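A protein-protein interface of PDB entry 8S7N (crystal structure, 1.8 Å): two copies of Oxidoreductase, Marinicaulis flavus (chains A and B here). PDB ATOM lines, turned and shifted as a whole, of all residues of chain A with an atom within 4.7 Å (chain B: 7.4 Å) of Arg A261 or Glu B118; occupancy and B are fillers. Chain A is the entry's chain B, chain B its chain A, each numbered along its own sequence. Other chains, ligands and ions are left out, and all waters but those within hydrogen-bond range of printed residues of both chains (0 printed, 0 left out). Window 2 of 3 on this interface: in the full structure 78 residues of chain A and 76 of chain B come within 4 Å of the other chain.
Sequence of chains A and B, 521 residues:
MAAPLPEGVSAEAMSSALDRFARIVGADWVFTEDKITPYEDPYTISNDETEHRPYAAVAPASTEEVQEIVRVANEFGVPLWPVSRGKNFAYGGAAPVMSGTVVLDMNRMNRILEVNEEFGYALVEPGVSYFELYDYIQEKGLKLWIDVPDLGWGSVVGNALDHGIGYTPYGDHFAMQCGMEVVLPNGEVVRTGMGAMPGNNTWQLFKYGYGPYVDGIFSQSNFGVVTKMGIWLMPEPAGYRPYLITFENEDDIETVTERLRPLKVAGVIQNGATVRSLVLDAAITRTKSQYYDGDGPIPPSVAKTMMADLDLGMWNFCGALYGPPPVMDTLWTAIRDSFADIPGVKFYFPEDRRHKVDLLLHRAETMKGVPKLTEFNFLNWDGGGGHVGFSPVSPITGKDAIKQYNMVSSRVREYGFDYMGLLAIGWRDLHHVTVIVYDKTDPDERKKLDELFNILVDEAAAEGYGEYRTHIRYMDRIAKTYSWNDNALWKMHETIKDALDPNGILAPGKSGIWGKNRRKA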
ATOM      1  N   THR A 257      19.319  38.205  21.278  1.00  0.00           N
ATOM      2  CA  THR A 257      19.302  36.724  21.425  1.00  0.00           C
ATOM      3  C   THR A 257      17.898  36.261  21.810  1.00  0.00           C
ATOM      4  O   THR A 257      17.414  35.262  21.260  1.00  0.00           O
ATOM      5  CB  THR A 257      20.353  36.244  22.412  1.00  0.00           C
ATOM      6  OG1 THR A 257      21.596  36.711  21.902  1.00  0.00           O
ATOM      7  CG2 THR A 257      20.327  34.731  22.550  1.00  0.00           C
ATOM      8  N   GLU A 258      17.218  36.964  22.720  1.00  0.00           N
ATOM      9  CA  GLU A 258      15.814  36.639  23.066  1.00  0.00           C
ATOM     10  C   GLU A 258      14.940  36.638  21.812  1.00  0.00           C
ATOM     11  O   GLU A 258      14.026  35.766  21.684  1.00  0.00           O
ATOM     12  CB  GLU A 258      15.273  37.647  24.109  1.00  0.00           C
ATOM     13  CG  GLU A 258      15.876  37.402  25.488  1.00  0.00           C
ATOM     14  CD  GLU A 258      15.566  36.011  26.040  1.00  0.00           C
ATOM     15  OE1 GLU A 258      14.399  35.798  26.306  1.00  0.00           O
ATOM     16  OE2 GLU A 258      16.469  35.132  26.149  1.00  0.00           O
ATOM     17  N   ARG A 259      15.112  37.622  20.942  1.00  0.00           N
ATOM     18  CA  ARG A 259      14.298  37.746  19.710  1.00  0.00           C
ATOM     19  C   ARG A 259      14.691  36.696  18.662  1.00  0.00           C
ATOM     20  O   ARG A 259      13.802  36.244  17.919  1.00  0.00           O
ATOM     21  CB  ARG A 259      14.430  39.163  19.137  1.00  0.00           C
ATOM     22  CG  ARG A 259      13.810  40.250  20.008  1.00  0.00           C
ATOM     23  CD  ARG A 259      14.631  41.519  19.904  1.00  0.00           C
ATOM     24  NE  ARG A 259      14.300  42.517  20.935  1.00  0.00           N
ATOM     25  CZ  ARG A 259      13.446  43.523  20.790  1.00  0.00           C
ATOM     26  NH1 ARG A 259      12.820  43.726  19.639  1.00  0.00           N
ATOM     27  NH2 ARG A 259      13.265  44.354  21.806  1.00  0.00           N
ATOM     28  N   LEU A 260      15.969  36.299  18.588  1.00  0.00           N
ATOM     29  CA  LEU A 260      16.427  35.258  17.617  1.00  0.00           C
ATOM     30  C   LEU A 260      15.805  33.900  17.951  1.00  0.00           C
ATOM     31  O   LEU A 260      15.519  33.137  17.041  1.00  0.00           O
ATOM     32  CB  LEU A 260      17.954  35.117  17.687  1.00  0.00           C
ATOM     33  CG  LEU A 260      18.762  36.259  17.107  1.00  0.00           C
ATOM     34  CD1 LEU A 260      20.244  36.088  17.400  1.00  0.00           C
ATOM     35  CD2 LEU A 260      18.547  36.319  15.602  1.00  0.00           C
ATOM     36  N   ARG A 261      15.647  33.583  19.233  1.00  0.00           N
ATOM     37  CA  ARG A 261      15.230  32.223  19.650  1.00  0.00           C
ATOM     38  C   ARG A 261      13.943  31.786  18.943  1.00  0.00           C
ATOM     39  O   ARG A 261      13.978  30.765  18.276  1.00  0.00           O
ATOM     40  CB  ARG A 261      15.110  32.117  21.174  1.00  0.00           C
ATOM     41  CG  ARG A 261      14.668  30.725  21.607  1.00  0.00           C
ATOM     42  CD  ARG A 261      14.503  30.663  23.120  1.00  0.00           C
ATOM     43  NE  ARG A 261      13.679  31.692  23.731  1.00  0.00           N
ATOM     44  CZ  ARG A 261      14.099  32.694  24.508  1.00  0.00           C
ATOM     45  NH1 ARG A 261      15.372  32.881  24.807  1.00  0.00           N
ATOM     46  NH2 ARG A 261      13.228  33.562  24.966  1.00  0.00           N
ATOM     47  N   PRO A 262      12.767  32.446  19.071  1.00  0.00           N
ATOM     48  CA  PRO A 262      11.553  31.936  18.423  1.00  0.00           C
ATOM     49  C   PRO A 262      11.699  31.858  16.884  1.00  0.00           C
ATOM     50  O   PRO A 262      11.162  30.945  16.254  1.00  0.00           O
ATOM     51  CB  PRO A 262      10.449  32.913  18.907  1.00  0.00           C
ATOM     52  CG  PRO A 262      11.204  34.168  19.335  1.00  0.00           C
ATOM     53  CD  PRO A 262      12.511  33.636  19.876  1.00  0.00           C
ATOM     54  N   LEU A 263      12.398  32.823  16.291  1.00  0.00           N
ATOM     55  CA  LEU A 263      12.617  32.846  14.812  1.00  0.00           C
ATOM     56  C   LEU A 263      13.432  31.617  14.400  1.00  0.00           C
ATOM     57  O   LEU A 263      13.111  31.041  13.373  1.00  0.00           O
ATOM     58  CB  LEU A 263      13.359  34.118  14.404  1.00  0.00           C
ATOM     59  CG  LEU A 263      12.601  35.422  14.645  1.00  0.00           C
ATOM     60  CD1 LEU A 263      13.549  36.558  14.388  1.00  0.00           C
ATOM     61  CD2 LEU A 263      11.358  35.484  13.752  1.00  0.00           C
ATOM     62  N   LYS A 264      14.488  31.266  15.136  1.00  0.00           N
ATOM     63  CA  LYS A 264      15.303  30.074  14.746  1.00  0.00           C
ATOM     64  C   LYS A 264      14.547  28.776  15.068  1.00  0.00           C
ATOM     65  O   LYS A 264      14.470  27.889  14.204  1.00  0.00           O
ATOM     66  CB  LYS A 264      16.675  30.123  15.401  1.00  0.00           C
ATOM     67  CG  LYS A 264      17.595  28.995  14.921  1.00  0.00           C
ATOM     68  CD  LYS A 264      17.985  29.204  13.449  1.00  0.00           C
ATOM     69  CE  LYS A 264      18.812  28.081  12.877  1.00  0.00           C
ATOM     70  NZ  LYS A 264      18.704  27.993  11.413  1.00  0.00           N
ATOM     71  N   VAL A 265      13.947  28.656  16.250  1.00  0.00           N
ATOM     72  CA  VAL A 265      13.287  27.385  16.649  1.00  0.00           C
ATOM     73  C   VAL A 265      12.184  27.048  15.622  1.00  0.00           C
ATOM     74  O   VAL A 265      11.980  25.841  15.348  1.00  0.00           O
ATOM     75  CB  VAL A 265      12.791  27.474  18.115  1.00  0.00           C
ATOM     76  CG1 VAL A 265      11.975  26.261  18.496  1.00  0.00           C
ATOM     77  CG2 VAL A 265      13.924  27.653  19.118  1.00  0.00           C
ATOM     78  N   ILE A 396      20.203  29.571  23.152  1.00  0.00           N
ATOM     79  CA  ILE A 396      19.727  30.826  22.484  1.00  0.00           C
ATOM     80  C   ILE A 396      18.917  31.620  23.503  1.00  0.00           C
ATOM     81  O   ILE A 396      17.677  31.733  23.394  1.00  0.00           O
ATOM     82  CB  ILE A 396      18.967  30.581  21.181  1.00  0.00           C
ATOM     83  CG1 ILE A 396      19.675  29.578  20.285  1.00  0.00           C
ATOM     84  CG2 ILE A 396      18.821  31.940  20.480  1.00  0.00           C
ATOM     85  CD1 ILE A 396      18.857  29.180  19.059  1.00  0.00           C
ATOM     86  N   THR A 397      19.620  32.141  24.499  1.00  0.00           N
ATOM     87  CA  THR A 397      19.020  32.921  25.588  1.00  0.00           C
ATOM     88  C   THR A 397      19.897  34.160  25.798  1.00  0.00           C
ATOM     89  O   THR A 397      21.146  33.991  25.886  1.00  0.00           O
ATOM     90  CB  THR A 397      18.978  32.052  26.862  1.00  0.00           C
ATOM     91  OG1 THR A 397      18.193  30.859  26.644  1.00  0.00           O
ATOM     92  CG2 THR A 397      18.433  32.830  28.025  1.00  0.00           C
ATOM     93  N   VAL B 115       8.946  19.845  29.536  1.00  0.00           N
ATOM     94  CA  VAL B 115       8.524  20.256  28.179  1.00  0.00           C
ATOM     95  C   VAL B 115       8.763  21.735  28.072  1.00  0.00           C
ATOM     96  O   VAL B 115       8.240  22.462  28.936  1.00  0.00           O
ATOM     97  CB  VAL B 115       7.062  19.947  27.874  1.00  0.00           C
ATOM     98  CG1 VAL B 115       6.713  20.400  26.456  1.00  0.00           C
ATOM     99  CG2 VAL B 115       6.750  18.486  28.036  1.00  0.00           C
ATOM    100  N   ASN B 116       9.616  22.130  27.133  1.00  0.00           N
ATOM    101  CA  ASN B 116      10.122  23.515  27.055  1.00  0.00           C
ATOM    102  C   ASN B 116       9.494  24.171  25.815  1.00  0.00           C
ATOM    103  O   ASN B 116       9.853  23.805  24.697  1.00  0.00           O
ATOM    104  CB  ASN B 116      11.647  23.527  27.083  1.00  0.00           C
ATOM    105  CG  ASN B 116      12.205  24.920  27.197  1.00  0.00           C
ATOM    106  OD1 ASN B 116      11.852  25.815  26.419  1.00  0.00           O
ATOM    107  ND2 ASN B 116      13.043  25.132  28.179  1.00  0.00           N
ATOM    108  N   GLU B 117       8.553  25.080  26.023  1.00  0.00           N
ATOM    109  CA  GLU B 117       7.840  25.755  24.911  1.00  0.00           C
ATOM    110  C   GLU B 117       8.818  26.646  24.127  1.00  0.00           C
ATOM    111  O   GLU B 117       8.821  26.579  22.874  1.00  0.00           O
ATOM    112  CB  GLU B 117       6.642  26.531  25.455  1.00  0.00           C
ATOM    113  CG  GLU B 117       5.842  27.181  24.353  1.00  0.00           C
ATOM    114  CD  GLU B 117       4.737  28.083  24.885  1.00  0.00           C
ATOM    115  OE1 GLU B 117       5.061  29.082  25.451  1.00  0.00           O
ATOM    116  OE2 GLU B 117       3.604  27.732  24.793  1.00  0.00           O
ATOM    117  N   GLU B 118       9.640  27.439  24.792  1.00  0.00           N
ATOM    118  CA  GLU B 118      10.380  28.478  24.053  1.00  0.00           C
ATOM    119  C   GLU B 118      11.524  27.813  23.274  1.00  0.00           C
ATOM    120  O   GLU B 118      11.846  28.338  22.200  1.00  0.00           O
ATOM    121  CB  GLU B 118      10.803  29.618  24.956  1.00  0.00           C
ATOM    122  CG  GLU B 118      11.854  29.226  25.918  1.00  0.00           C
ATOM    123  CD  GLU B 118      12.138  30.363  26.884  1.00  0.00           C
ATOM    124  OE1 GLU B 118      11.327  31.325  26.878  1.00  0.00           O
ATOM    125  OE2 GLU B 118      13.172  30.289  27.610  1.00  0.00           O
ATOM    126  N   PHE B 119      12.070  26.685  23.728  1.00  0.00           N
ATOM    127  CA  PHE B 119      13.080  25.950  22.919  1.00  0.00           C
ATOM    128  C   PHE B 119      12.505  24.775  22.135  1.00  0.00           C
ATOM    129  O   PHE B 119      13.266  24.193  21.337  1.00  0.00           O
ATOM    130  CB  PHE B 119      14.241  25.494  23.779  1.00  0.00           C
ATOM    131  CG  PHE B 119      15.192  26.604  24.072  1.00  0.00           C
ATOM    132  CD1 PHE B 119      16.080  27.029  23.078  1.00  0.00           C
ATOM    133  CD2 PHE B 119      15.262  27.156  25.333  1.00  0.00           C
ATOM    134  CE1 PHE B 119      17.021  28.014  23.345  1.00  0.00           C
ATOM    135  CE2 PHE B 119      16.179  28.165  25.592  1.00  0.00           C
ATOM    136  CZ  PHE B 119      17.024  28.602  24.598  1.00  0.00           C
ATOM    137  N   GLY B 120      11.231  24.451  22.292  1.00  0.00           N
ATOM    138  CA  GLY B 120      10.588  23.358  21.563  1.00  0.00           C
ATOM    139  C   GLY B 120      11.274  22.042  21.800  1.00  0.00           C
ATOM    140  O   GLY B 120      11.898  21.482  20.873  1.00  0.00           O
ATOM    141  N   TYR B 121      11.185  21.515  23.009  1.00  0.00           N
ATOM    142  CA  TYR B 121      11.717  20.167  23.287  1.00  0.00           C
ATOM    143  C   TYR B 121      10.968  19.533  24.452  1.00  0.00           C
ATOM    144  O   TYR B 121      10.331  20.232  25.282  1.00  0.00           O
ATOM    145  CB  TYR B 121      13.230  20.199  23.528  1.00  0.00           C
ATOM    146  CG  TYR B 121      13.711  20.730  24.851  1.00  0.00           C
ATOM    147  CD1 TYR B 121      13.532  20.050  26.052  1.00  0.00           C
ATOM    148  CD2 TYR B 121      14.317  21.969  24.886  1.00  0.00           C
ATOM    149  CE1 TYR B 121      14.051  20.564  27.229  1.00  0.00           C
ATOM    150  CE2 TYR B 121      14.819  22.500  26.058  1.00  0.00           C
ATOM    151  CZ  TYR B 121      14.694  21.785  27.226  1.00  0.00           C
ATOM    152  OH  TYR B 121      15.160  22.392  28.353  1.00  0.00           O
ATOM    153  N   LEU B 142       0.666  24.645  26.201  1.00  0.00           N
ATOM    154  CA  LEU B 142       1.961  24.872  25.504  1.00  0.00           C
ATOM    155  C   LEU B 142       1.710  24.871  23.991  1.00  0.00           C
ATOM    156  O   LEU B 142       0.955  24.005  23.469  1.00  0.00           O
ATOM    157  CB  LEU B 142       2.999  23.826  25.956  1.00  0.00           C
ATOM    158  CG  LEU B 142       3.307  23.808  27.444  1.00  0.00           C
ATOM    159  CD1 LEU B 142       4.497  22.955  27.733  1.00  0.00           C
ATOM    160  CD2 LEU B 142       3.561  25.206  27.997  1.00  0.00           C
ATOM    161  N   LEU B 144       2.968  23.827  21.163  1.00  0.00           N
ATOM    162  CA  LEU B 144       3.867  22.814  20.593  1.00  0.00           C
ATOM    163  C   LEU B 144       3.006  21.729  20.010  1.00  0.00           C
ATOM    164  O   LEU B 144       2.023  21.362  20.628  1.00  0.00           O
ATOM    165  CB  LEU B 144       4.748  22.190  21.669  1.00  0.00           C
ATOM    166  CG  LEU B 144       5.686  23.145  22.377  1.00  0.00           C
ATOM    167  CD1 LEU B 144       6.306  22.444  23.584  1.00  0.00           C
ATOM    168  CD2 LEU B 144       6.731  23.680  21.426  1.00  0.00           C
ATOM    169  N   LEU B 205      19.565  21.040  23.731  1.00  0.00           N
ATOM    170  CA  LEU B 205      19.728  22.163  22.767  1.00  0.00           C
ATOM    171  C   LEU B 205      20.816  21.856  21.710  1.00  0.00           C
ATOM    172  O   LEU B 205      20.730  22.388  20.610  1.00  0.00           O
ATOM    173  CB  LEU B 205      20.075  23.413  23.569  1.00  0.00           C
ATOM    174  CG  LEU B 205      19.027  23.859  24.600  1.00  0.00           C
ATOM    175  CD1 LEU B 205      19.382  25.225  25.143  1.00  0.00           C
ATOM    176  CD2 LEU B 205      17.635  23.885  23.971  1.00  0.00           C
ATOM    177  N   PRO B 235       7.221  24.023  17.123  1.00  0.00           N
ATOM    178  CA  PRO B 235       6.349  25.141  17.500  1.00  0.00           C
ATOM    179  C   PRO B 235       5.032  25.040  16.700  1.00  0.00           C
ATOM    180  O   PRO B 235       5.046  24.729  15.531  1.00  0.00           O
ATOM    181  CB  PRO B 235       7.138  26.417  17.185  1.00  0.00           C
ATOM    182  CG  PRO B 235       8.555  25.932  17.147  1.00  0.00           C
ATOM    183  CD  PRO B 235       8.521  24.495  16.645  1.00  0.00           C
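Arg A261 touches just these residues of chain B: Glu B118 (3.5 Å) and Phe B119 (3.6 Å). Printed residues of chain B within 4 Å of Val A265: Glu B118 (3.8 Å), Phe B119 (3.7 Å) and Pro B235 (3.7 Å). Printed residues of chain B within 4 Å of Ile A396: Phe B119 (3.4 Å). Printed residues of chain B within 4 Å of Thr A397: Phe B119. Of chain A, only Arg A261 (3.5 Å) and Val A265 (3.8 Å) come within 4 Å of Glu B118. Of the printed residues of chain A, Phe B119 touches Arg A261, Val A265, Ile A396 and Thr A397. Of the printed residues of chain A, Pro B235 touches Val A265. The nearest residue of chain B that does not touch Arg A261 is Asn B116 (6.4 Å). The nearest printed residue of chain A that does not touch Glu B118 is Thr A397 (5.1 Å). The nearest printed residue of chain A that does not touch Phe B119 is Glu A258 (6.7 Å).
NH2 of Arg A261 is in salt-bridge range of OE1 of Glu B118, 3.5 Å away.
No position is printed for both chains.
Among the printed residues, pairs that only touch across the chains: Arg A261 with Phe B119, Val A265 with Glu B118, Val A265 with Phe B119, Val A265 with Pro B235, Ile A396 with Phe B119 and Thr A397 with Phe B119.
Printed residues of chain A that touch a printed residue of chain B: Arg A261, Val A265, Ile A396 and Thr A397. Among the printed residues, 7 pairs touch across the chains. Among the printed residues, Asp or Glu carboxylates within 4 Å of a Lys or Arg side-chain nitrogen of the other chain: Arg A261 with Glu B118 (3.5 Å).
The side-chain amide oxygen (OD1) of Asn B116 is in hydrogen-bond range of the backbone NH (N) of Glu B118 (3.2 Å). The backbone NH (N) of Phe B119 sits at hydrogen-bond distance from the side-chain amide oxygen (OD1) of Asn B116. The side-chain carboxylate (OE2) of Glu A258 is in salt-bridge range of the guanidinium group (NH1) of Arg A261, 2.8 Å away. The guanidinium group (NH1) of Arg A261 sits at hydrogen-bond distance from the backbone carbonyl oxygen (O) of Ile A396, at 2.9 Å.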
